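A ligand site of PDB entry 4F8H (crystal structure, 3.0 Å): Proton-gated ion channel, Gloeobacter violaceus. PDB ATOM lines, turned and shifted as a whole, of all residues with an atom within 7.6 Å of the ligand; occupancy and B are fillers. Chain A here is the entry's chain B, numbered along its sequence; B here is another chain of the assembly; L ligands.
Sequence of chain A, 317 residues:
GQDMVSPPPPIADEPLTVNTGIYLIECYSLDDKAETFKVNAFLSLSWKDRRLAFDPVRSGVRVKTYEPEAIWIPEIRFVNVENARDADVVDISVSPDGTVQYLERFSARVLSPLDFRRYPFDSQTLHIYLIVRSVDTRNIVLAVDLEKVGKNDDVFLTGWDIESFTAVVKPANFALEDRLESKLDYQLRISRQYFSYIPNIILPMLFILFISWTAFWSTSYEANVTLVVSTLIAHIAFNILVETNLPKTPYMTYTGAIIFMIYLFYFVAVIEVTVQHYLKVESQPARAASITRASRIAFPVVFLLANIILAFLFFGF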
ATOM      1  N   TYR A  23     -10.932  -4.449  13.710  1.00  0.00           N
ATOM      2  CA  TYR A  23     -11.551  -4.637  15.032  1.00  0.00           C
ATOM      3  C   TYR A  23     -12.479  -5.842  14.989  1.00  0.00           C
ATOM      4  O   TYR A  23     -13.579  -5.752  14.414  1.00  0.00           O
ATOM      5  CB  TYR A  23     -12.312  -3.395  15.473  1.00  0.00           C
ATOM      6  CG  TYR A  23     -13.016  -3.510  16.806  1.00  0.00           C
ATOM      7  CD1 TYR A  23     -12.352  -3.212  17.994  1.00  0.00           C
ATOM      8  CD2 TYR A  23     -14.342  -3.910  16.897  1.00  0.00           C
ATOM      9  CE1 TYR A  23     -12.996  -3.305  19.218  1.00  0.00           C
ATOM     10  CE2 TYR A  23     -14.993  -4.011  18.119  1.00  0.00           C
ATOM     11  CZ  TYR A  23     -14.305  -3.702  19.281  1.00  0.00           C
ATOM     12  OH  TYR A  23     -14.937  -3.793  20.512  1.00  0.00           O
ATOM     13  N   LEU A  24     -12.033  -6.946  15.579  1.00  0.00           N
ATOM     14  CA  LEU A  24     -12.781  -8.204  15.544  1.00  0.00           C
ATOM     15  C   LEU A  24     -14.064  -8.058  16.325  1.00  0.00           C
ATOM     16  O   LEU A  24     -14.088  -7.489  17.414  1.00  0.00           O
ATOM     17  CB  LEU A  24     -11.948  -9.324  16.130  1.00  0.00           C
ATOM     18  CG  LEU A  24     -10.539  -9.438  15.527  1.00  0.00           C
ATOM     19  CD1 LEU A  24      -9.676 -10.369  16.326  1.00  0.00           C
ATOM     20  CD2 LEU A  24     -10.590  -9.873  14.066  1.00  0.00           C
ATOM     21  N   ILE A  25     -15.152  -8.555  15.743  1.00  0.00           N
ATOM     22  CA  ILE A  25     -16.445  -8.566  16.404  1.00  0.00           C
ATOM     23  C   ILE A  25     -16.764 -10.014  16.744  1.00  0.00           C
ATOM     24  O   ILE A  25     -17.310 -10.297  17.807  1.00  0.00           O
ATOM     25  CB  ILE A  25     -17.539  -7.977  15.500  1.00  0.00           C
ATOM     26  CG1 ILE A  25     -17.225  -6.526  15.167  1.00  0.00           C
ATOM     27  CG2 ILE A  25     -18.903  -8.127  16.157  1.00  0.00           C
ATOM     28  CD1 ILE A  25     -17.986  -6.021  13.938  1.00  0.00           C
ATOM     29  N   PHE A  42     -14.646  -5.148  11.790  1.00  0.00           N
ATOM     30  CA  PHE A  42     -14.567  -3.825  11.152  1.00  0.00           C
ATOM     31  C   PHE A  42     -13.236  -3.721  10.465  1.00  0.00           C
ATOM     32  O   PHE A  42     -12.203  -3.976  11.089  1.00  0.00           O
ATOM     33  CB  PHE A  42     -14.630  -2.699  12.179  1.00  0.00           C
ATOM     34  CG  PHE A  42     -16.023  -2.301  12.551  1.00  0.00           C
ATOM     35  CD1 PHE A  42     -17.034  -2.298  11.597  1.00  0.00           C
ATOM     36  CD2 PHE A  42     -16.333  -1.936  13.852  1.00  0.00           C
ATOM     37  CE1 PHE A  42     -18.321  -1.934  11.943  1.00  0.00           C
ATOM     38  CE2 PHE A  42     -17.619  -1.559  14.193  1.00  0.00           C
ATOM     39  CZ  PHE A  42     -18.607  -1.564  13.244  1.00  0.00           C
ATOM     40  N   ARG A 105     -17.790  -3.243   7.395  1.00  0.00           N
ATOM     41  CA  ARG A 105     -17.851  -4.433   8.236  1.00  0.00           C
ATOM     42  C   ARG A 105     -17.807  -5.644   7.323  1.00  0.00           C
ATOM     43  O   ARG A 105     -18.616  -5.770   6.400  1.00  0.00           O
ATOM     44  CB  ARG A 105     -19.115  -4.452   9.090  1.00  0.00           C
ATOM     45  CG  ARG A 105     -19.215  -5.687   9.922  1.00  0.00           C
ATOM     46  CD  ARG A 105     -20.288  -5.591  10.993  1.00  0.00           C
ATOM     47  NE  ARG A 105     -20.530  -6.908  11.565  1.00  0.00           N
ATOM     48  CZ  ARG A 105     -21.465  -7.181  12.451  1.00  0.00           C
ATOM     49  NH1 ARG A 105     -22.270  -6.220  12.879  1.00  0.00           N
ATOM     50  NH2 ARG A 105     -21.605  -8.405  12.912  1.00  0.00           N
ATOM     51  N   LYS A 151     -10.472  -5.830  19.549  1.00  0.00           N
ATOM     52  CA  LYS A 151     -11.494  -6.863  19.520  1.00  0.00           C
ATOM     53  C   LYS A 151     -12.401  -6.612  20.706  1.00  0.00           C
ATOM     54  O   LYS A 151     -11.929  -6.188  21.755  1.00  0.00           O
ATOM     55  CB  LYS A 151     -10.836  -8.223  19.696  1.00  0.00           C
ATOM     56  CG  LYS A 151     -10.064  -8.309  20.998  1.00  0.00           C
ATOM     57  CD  LYS A 151      -9.148  -9.516  21.082  1.00  0.00           C
ATOM     58  CE  LYS A 151      -9.025  -9.958  22.522  1.00  0.00           C
ATOM     59  NZ  LYS A 151     -10.388 -10.087  23.133  1.00  0.00           N
ATOM     60  N   ASN A 152     -13.701  -6.855  20.552  1.00  0.00           N
ATOM     61  CA  ASN A 152     -14.590  -6.652  21.693  1.00  0.00           C
ATOM     62  C   ASN A 152     -14.458  -7.777  22.720  1.00  0.00           C
ATOM     63  O   ASN A 152     -13.954  -8.859  22.418  1.00  0.00           O
ATOM     64  CB  ASN A 152     -16.034  -6.405  21.249  1.00  0.00           C
ATOM     65  CG  ASN A 152     -16.766  -7.670  20.890  1.00  0.00           C
ATOM     66  OD1 ASN A 152     -17.595  -8.160  21.647  1.00  0.00           O
ATOM     67  ND2 ASN A 152     -16.477  -8.198  19.697  1.00  0.00           N
ATOM     68  N   ASP A 153     -14.905  -7.505  23.938  1.00  0.00           N
ATOM     69  CA  ASP A 153     -14.692  -8.388  25.087  1.00  0.00           C
ATOM     70  C   ASP A 153     -15.452  -9.721  25.010  1.00  0.00           C
ATOM     71  O   ASP A 153     -15.053 -10.707  25.620  1.00  0.00           O
ATOM     72  CB  ASP A 153     -15.048  -7.660  26.378  1.00  0.00           C
ATOM     73  CG  ASP A 153     -14.338  -6.319  26.506  1.00  0.00           C
ATOM     74  OD1 ASP A 153     -13.137  -6.249  26.184  1.00  0.00           O
ATOM     75  OD2 ASP A 153     -14.995  -5.324  26.920  1.00  0.00           O
ATOM     76  N   ASP A 154     -16.542  -9.753  24.250  1.00  0.00           N
ATOM     77  CA  ASP A 154     -17.304 -10.975  24.019  1.00  0.00           C
ATOM     78  C   ASP A 154     -16.548 -12.017  23.175  1.00  0.00           C
ATOM     79  O   ASP A 154     -16.552 -13.205  23.522  1.00  0.00           O
ATOM     80  CB  ASP A 154     -18.638 -10.660  23.337  1.00  0.00           C
ATOM     81  CG  ASP A 154     -19.470  -9.675  24.113  1.00  0.00           C
ATOM     82  OD1 ASP A 154     -19.305  -9.620  25.352  1.00  0.00           O
ATOM     83  OD2 ASP A 154     -20.296  -8.967  23.477  1.00  0.00           O
ATOM     84  N   VAL A 155     -15.927 -11.567  22.092  1.00  0.00           N
ATOM     85  CA  VAL A 155     -15.277 -12.448  21.102  1.00  0.00           C
ATOM     86  C   VAL A 155     -14.845 -13.751  21.744  1.00  0.00           C
ATOM     87  O   VAL A 155     -13.817 -13.811  22.423  1.00  0.00           O
ATOM     88  CB  VAL A 155     -14.039 -11.800  20.450  1.00  0.00           C
ATOM     89  CG1 VAL A 155     -13.468 -12.707  19.390  1.00  0.00           C
ATOM     90  CG2 VAL A 155     -14.410 -10.462  19.837  1.00  0.00           C
ATOM     91  N   ARG B  77     -27.701  -2.797  12.525  1.00  0.00           N
ATOM     92  CA  ARG B  77     -27.029  -4.065  12.215  1.00  0.00           C
ATOM     93  C   ARG B  77     -27.067  -5.023  13.426  1.00  0.00           C
ATOM     94  O   ARG B  77     -27.160  -4.577  14.572  1.00  0.00           O
ATOM     95  CB  ARG B  77     -25.585  -3.816  11.726  1.00  0.00           C
ATOM     96  CG  ARG B  77     -25.475  -2.941  10.473  1.00  0.00           C
ATOM     97  CD  ARG B  77     -24.020  -2.645  10.115  1.00  0.00           C
ATOM     98  NE  ARG B  77     -23.191  -2.561  11.318  1.00  0.00           N
ATOM     99  CZ  ARG B  77     -22.872  -1.426  11.936  1.00  0.00           C
ATOM    100  NH1 ARG B  77     -23.287  -0.248  11.452  1.00  0.00           N
ATOM    101  NH2 ARG B  77     -22.121  -1.484  13.042  1.00  0.00           N
ATOM    102  N   PHE B  78     -27.007  -6.328  13.165  1.00  0.00           N
ATOM    103  CA  PHE B  78     -26.914  -7.311  14.259  1.00  0.00           C
ATOM    104  C   PHE B  78     -25.465  -7.513  14.661  1.00  0.00           C
ATOM    105  O   PHE B  78     -24.595  -7.607  13.811  1.00  0.00           O
ATOM    106  CB  PHE B  78     -27.532  -8.660  13.887  1.00  0.00           C
ATOM    107  CG  PHE B  78     -29.021  -8.639  13.783  1.00  0.00           C
ATOM    108  CD1 PHE B  78     -29.800  -8.799  14.914  1.00  0.00           C
ATOM    109  CD2 PHE B  78     -29.650  -8.452  12.564  1.00  0.00           C
ATOM    110  CE1 PHE B  78     -31.179  -8.783  14.825  1.00  0.00           C
ATOM    111  CE2 PHE B  78     -31.029  -8.437  12.475  1.00  0.00           C
ATOM    112  CZ  PHE B  78     -31.790  -8.598  13.606  1.00  0.00           C
ATOM    113  N   VAL B  79     -25.206  -7.566  15.962  1.00  0.00           N
ATOM    114  CA  VAL B  79     -23.834  -7.722  16.407  1.00  0.00           C
ATOM    115  C   VAL B  79     -23.346  -9.157  16.273  1.00  0.00           C
ATOM    116  O   VAL B  79     -22.291  -9.385  15.703  1.00  0.00           O
ATOM    117  CB  VAL B  79     -23.673  -7.344  17.868  1.00  0.00           C
ATOM    118  CG1 VAL B  79     -22.251  -7.645  18.281  1.00  0.00           C
ATOM    119  CG2 VAL B  79     -24.019  -5.883  18.065  1.00  0.00           C
ATOM    120  N   ASN B  80     -24.103 -10.098  16.810  1.00  0.00           N
ATOM    121  CA  ASN B  80     -23.663 -11.487  16.869  1.00  0.00           C
ATOM    122  C   ASN B  80     -24.280 -12.387  15.807  1.00  0.00           C
ATOM    123  O   ASN B  80     -25.008 -13.334  16.106  1.00  0.00           O
ATOM    124  CB  ASN B  80     -23.890 -12.071  18.265  1.00  0.00           C
ATOM    125  CG  ASN B  80     -25.362 -12.132  18.664  1.00  0.00           C
ATOM    126  OD1 ASN B  80     -26.080 -11.148  18.623  1.00  0.00           O
ATOM    127  ND2 ASN B  80     -25.801 -13.323  19.054  1.00  0.00           N
ATOM    128  N   TYR B 129     -28.408  -9.331  19.521  1.00  0.00           N
ATOM    129  CA  TYR B 129     -28.029  -7.928  19.792  1.00  0.00           C
ATOM    130  C   TYR B 129     -28.204  -7.012  18.577  1.00  0.00           C
ATOM    131  O   TYR B 129     -27.504  -7.184  17.574  1.00  0.00           O
ATOM    132  CB  TYR B 129     -26.560  -7.807  20.236  1.00  0.00           C
ATOM    133  CG  TYR B 129     -26.239  -8.478  21.538  1.00  0.00           C
ATOM    134  CD1 TYR B 129     -26.673  -7.958  22.734  1.00  0.00           C
ATOM    135  CD2 TYR B 129     -25.469  -9.639  21.563  1.00  0.00           C
ATOM    136  CE1 TYR B 129     -26.365  -8.573  23.939  1.00  0.00           C
ATOM    137  CE2 TYR B 129     -25.155 -10.257  22.760  1.00  0.00           C
ATOM    138  CZ  TYR B 129     -25.607  -9.734  23.942  1.00  0.00           C
ATOM    139  OH  TYR B 129     -25.304 -10.354  25.131  1.00  0.00           O
ATOM    140  N   ILE B 131     -27.558  -3.349  16.982  1.00  0.00           N
ATOM    141  CA  ILE B 131     -26.676  -2.203  17.201  1.00  0.00           C
ATOM    142  C   ILE B 131     -26.870  -1.124  16.136  1.00  0.00           C
ATOM    143  O   ILE B 131     -27.299  -1.395  14.999  1.00  0.00           O
ATOM    144  CB  ILE B 131     -25.198  -2.637  17.269  1.00  0.00           C
ATOM    145  CG1 ILE B 131     -24.435  -1.790  18.288  1.00  0.00           C
ATOM    146  CG2 ILE B 131     -24.558  -2.581  15.903  1.00  0.00           C
ATOM    147  CD1 ILE B 131     -22.974  -2.160  18.382  1.00  0.00           C
ATOM    148  N   ALA B 172     -27.288  -0.324  25.844  1.00  0.00           N
ATOM    149  CA  ALA B 172     -25.940  -0.075  26.315  1.00  0.00           C
ATOM    150  C   ALA B 172     -25.291   0.846  25.307  1.00  0.00           C
ATOM    151  O   ALA B 172     -25.015   0.426  24.176  1.00  0.00           O
ATOM    152  CB  ALA B 172     -25.164  -1.350  26.421  1.00  0.00           C
ATOM    153  N   ASN B 173     -25.071   2.097  25.700  1.00  0.00           N
ATOM    154  CA  ASN B 173     -24.372   3.051  24.856  1.00  0.00           C
ATOM    155  C   ASN B 173     -22.896   3.069  25.247  1.00  0.00           C
ATOM    156  O   ASN B 173     -22.547   2.933  26.427  1.00  0.00           O
ATOM    157  CB  ASN B 173     -24.985   4.447  24.996  1.00  0.00           C
ATOM    158  CG  ASN B 173     -26.463   4.465  24.640  1.00  0.00           C
ATOM    159  OD1 ASN B 173     -26.919   3.726  23.766  1.00  0.00           O
ATOM    160  ND2 ASN B 173     -27.237   5.326  25.317  1.00  0.00           N
ATOM    161  N   PHE B 174     -22.025   3.217  24.251  1.00  0.00           N
ATOM    162  CA  PHE B 174     -20.586   3.163  24.478  1.00  0.00           C
ATOM    163  C   PHE B 174     -19.875   3.647  23.223  1.00  0.00           C
ATOM    164  O   PHE B 174     -20.502   3.787  22.169  1.00  0.00           O
ATOM    165  CB  PHE B 174     -20.124   1.753  24.836  1.00  0.00           C
ATOM    166  CG  PHE B 174     -20.256   0.762  23.715  1.00  0.00           C
ATOM    167  CD1 PHE B 174     -19.187   0.507  22.868  1.00  0.00           C
ATOM    168  CD2 PHE B 174     -21.447   0.089  23.488  1.00  0.00           C
ATOM    169  CE1 PHE B 174     -19.311  -0.397  21.820  1.00  0.00           C
ATOM    170  CE2 PHE B 174     -21.570  -0.804  22.448  1.00  0.00           C
ATOM    171  CZ  PHE B 174     -20.506  -1.058  21.623  1.00  0.00           C
ATOM    172  N   ALA B 175     -18.575   3.896  23.336  1.00  0.00           N
ATOM    173  CA  ALA B 175     -17.840   4.442  22.213  1.00  0.00           C
ATOM    174  C   ALA B 175     -16.982   3.372  21.545  1.00  0.00           C
ATOM    175  O   ALA B 175     -16.174   2.707  22.188  1.00  0.00           O
ATOM    176  CB  ALA B 175     -16.992   5.588  22.668  1.00  0.00           C
ATOM    177  N   LEU B 176     -17.163   3.211  20.237  1.00  0.00           N
ATOM    178  CA  LEU B 176     -16.399   2.240  19.484  1.00  0.00           C
ATOM    179  C   LEU B 176     -15.742   2.894  18.286  1.00  0.00           C
ATOM    180  O   LEU B 176     -16.418   3.237  17.317  1.00  0.00           O
ATOM    181  CB  LEU B 176     -17.289   1.090  19.028  1.00  0.00           C
ATOM    182  CG  LEU B 176     -16.595   0.004  18.211  1.00  0.00           C
ATOM    183  CD1 LEU B 176     -15.310  -0.407  18.926  1.00  0.00           C
ATOM    184  CD2 LEU B 176     -17.510  -1.186  18.027  1.00  0.00           C
ATOM    185  N   GLU B 181     -21.999   4.078  19.858  1.00  0.00           N
ATOM    186  CA  GLU B 181     -22.824   2.984  19.383  1.00  0.00           C
ATOM    187  C   GLU B 181     -23.916   2.651  20.394  1.00  0.00           C
ATOM    188  O   GLU B 181     -23.688   2.694  21.617  1.00  0.00           O
ATOM    189  CB  GLU B 181     -21.945   1.763  19.070  1.00  0.00           C
ATOM    190  CG  GLU B 181     -22.323   1.062  17.765  1.00  0.00           C
ATOM    191  CD  GLU B 181     -21.141   0.773  16.857  1.00  0.00           C
ATOM    192  OE1 GLU B 181     -20.052   1.346  17.094  1.00  0.00           O
ATOM    193  OE2 GLU B 181     -21.297  -0.040  15.903  1.00  0.00           O
ATOM    194  N   LYS B 183     -26.572  -0.324  21.612  1.00  0.00           N
ATOM    195  CA  LYS B 183     -26.752  -1.771  21.516  1.00  0.00           C
ATOM    196  C   LYS B 183     -27.920  -2.288  22.357  1.00  0.00           C
ATOM    197  O   LYS B 183     -27.995  -2.015  23.552  1.00  0.00           O
ATOM    198  CB  LYS B 183     -25.463  -2.482  21.936  1.00  0.00           C
ATOM    199  CG  LYS B 183     -25.434  -3.979  21.698  1.00  0.00           C
ATOM    200  CD  LYS B 183     -24.237  -4.635  22.406  1.00  0.00           C
ATOM    201  CE  LYS B 183     -24.448  -4.757  23.910  1.00  0.00           C
ATOM    202  NZ  LYS B 183     -23.280  -5.353  24.649  1.00  0.00           N
HETATM  203  C1  LIG L   1     -18.430  -4.022  19.496  1.00  0.00           C
HETATM  204  C2  LIG L   1     -19.570  -4.516  18.927  1.00  0.00           C
HETATM  205  C3  LIG L   1     -18.205  -4.127  20.873  1.00  0.00           C
HETATM  206  C4  LIG L   1     -20.486  -5.133  19.768  1.00  0.00           C
HETATM  207  C5  LIG L   1     -19.126  -4.729  21.731  1.00  0.00           C
HETATM  208  C6  LIG L   1     -20.291  -5.250  21.143  1.00  0.00           C
HETATM  209  C7  LIG L   1     -17.787  -3.701  23.680  1.00  0.00           C
HETATM  210  C8  LIG L   1     -18.407  -2.378  24.030  1.00  0.00           C
HETATM  211  C9  LIG L   1     -19.390  -2.557  25.219  1.00  0.00           C
HETATM  212  C10 LIG L   1     -20.565  -3.422  24.722  1.00  0.00           C
HETATM  213  C11 LIG L   1     -20.044  -4.808  24.238  1.00  0.00           C
HETATM  214  C12 LIG L   1     -18.799  -4.803  23.259  1.00  0.00           C
HETATM  215  C13 LIG L   1     -17.868  -6.494  24.867  1.00  0.00           C
HETATM  216  N1  LIG L   1     -18.131  -6.063  23.503  1.00  0.00           N
HETATM  217  O1  LIG L   1     -16.588  -3.903  23.749  1.00  0.00           O
HETATM  218 CL1  LIG L   1     -21.576  -6.094  22.134  1.00  0.00          CL
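The backbone carbonyl oxygen of Leu 24 is in hydrogen-bond range of the backbone NH of Asn 152 (3.2 Å). The backbone carbonyl oxygen of Phe 174 of chain B sits at hydrogen-bond distance from the backbone NH of Glu 181 of chain B, at 2.8 Å. ND2 of Asn 152 sits at hydrogen-bond distance from O of Ile 25 (2.9 Å). The backbone NH (N) of Asn 152 sits close to the side-chain hydroxyl (OH) of Tyr 23. OD1 of Asn 152 lies close to N of Asp 154, at 3.2 Å. The backbone NH (N) of Phe 42 is in hydrogen-bond range of the backbone carbonyl oxygen (O) of Tyr 23 (2.9 Å). NH2 of Arg 105 sits at hydrogen-bond distance from O of Val 79 of chain B, at 3.0 Å. The backbone NH (N) of Val 79 of chain B is in hydrogen-bond range of the backbone carbonyl oxygen (O) of Tyr 129 of chain B, at 2.8 Å.
The side-chain amide oxygen (OD1) of Asn 152 sits at hydrogen-bond distance from a nitrogen (N1) of the ligand (2.9 Å). A nitrogen (N1) of the ligand is in salt-bridge range of the side-chain carboxylate (OD2) of Asp 154, 3.6 Å away.
Merely in contact with the ligand: Lys 183 of chain B (3.0 Å), Phe 174 of chain B (3.1 Å), Asp 153 (3.3 Å), Tyr 23 (3.3 Å), Leu 176 of chain B (3.3 Å) and Val 79 of chain B (3.4 Å). Hydrophobic or aromatic side chains that line the ligand: Tyr 23, Val 79 of chain B, Phe 174 of chain B and Leu 176 of chain B. Of the 23 residues printed, 8 come within 4 Å of the ligand. Along chain A the residues within 4 Å of the ligand span positions 23 to 154. The nearest printed residue that does not touch the ligand is Ile 131 of chain B (4.1 Å).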
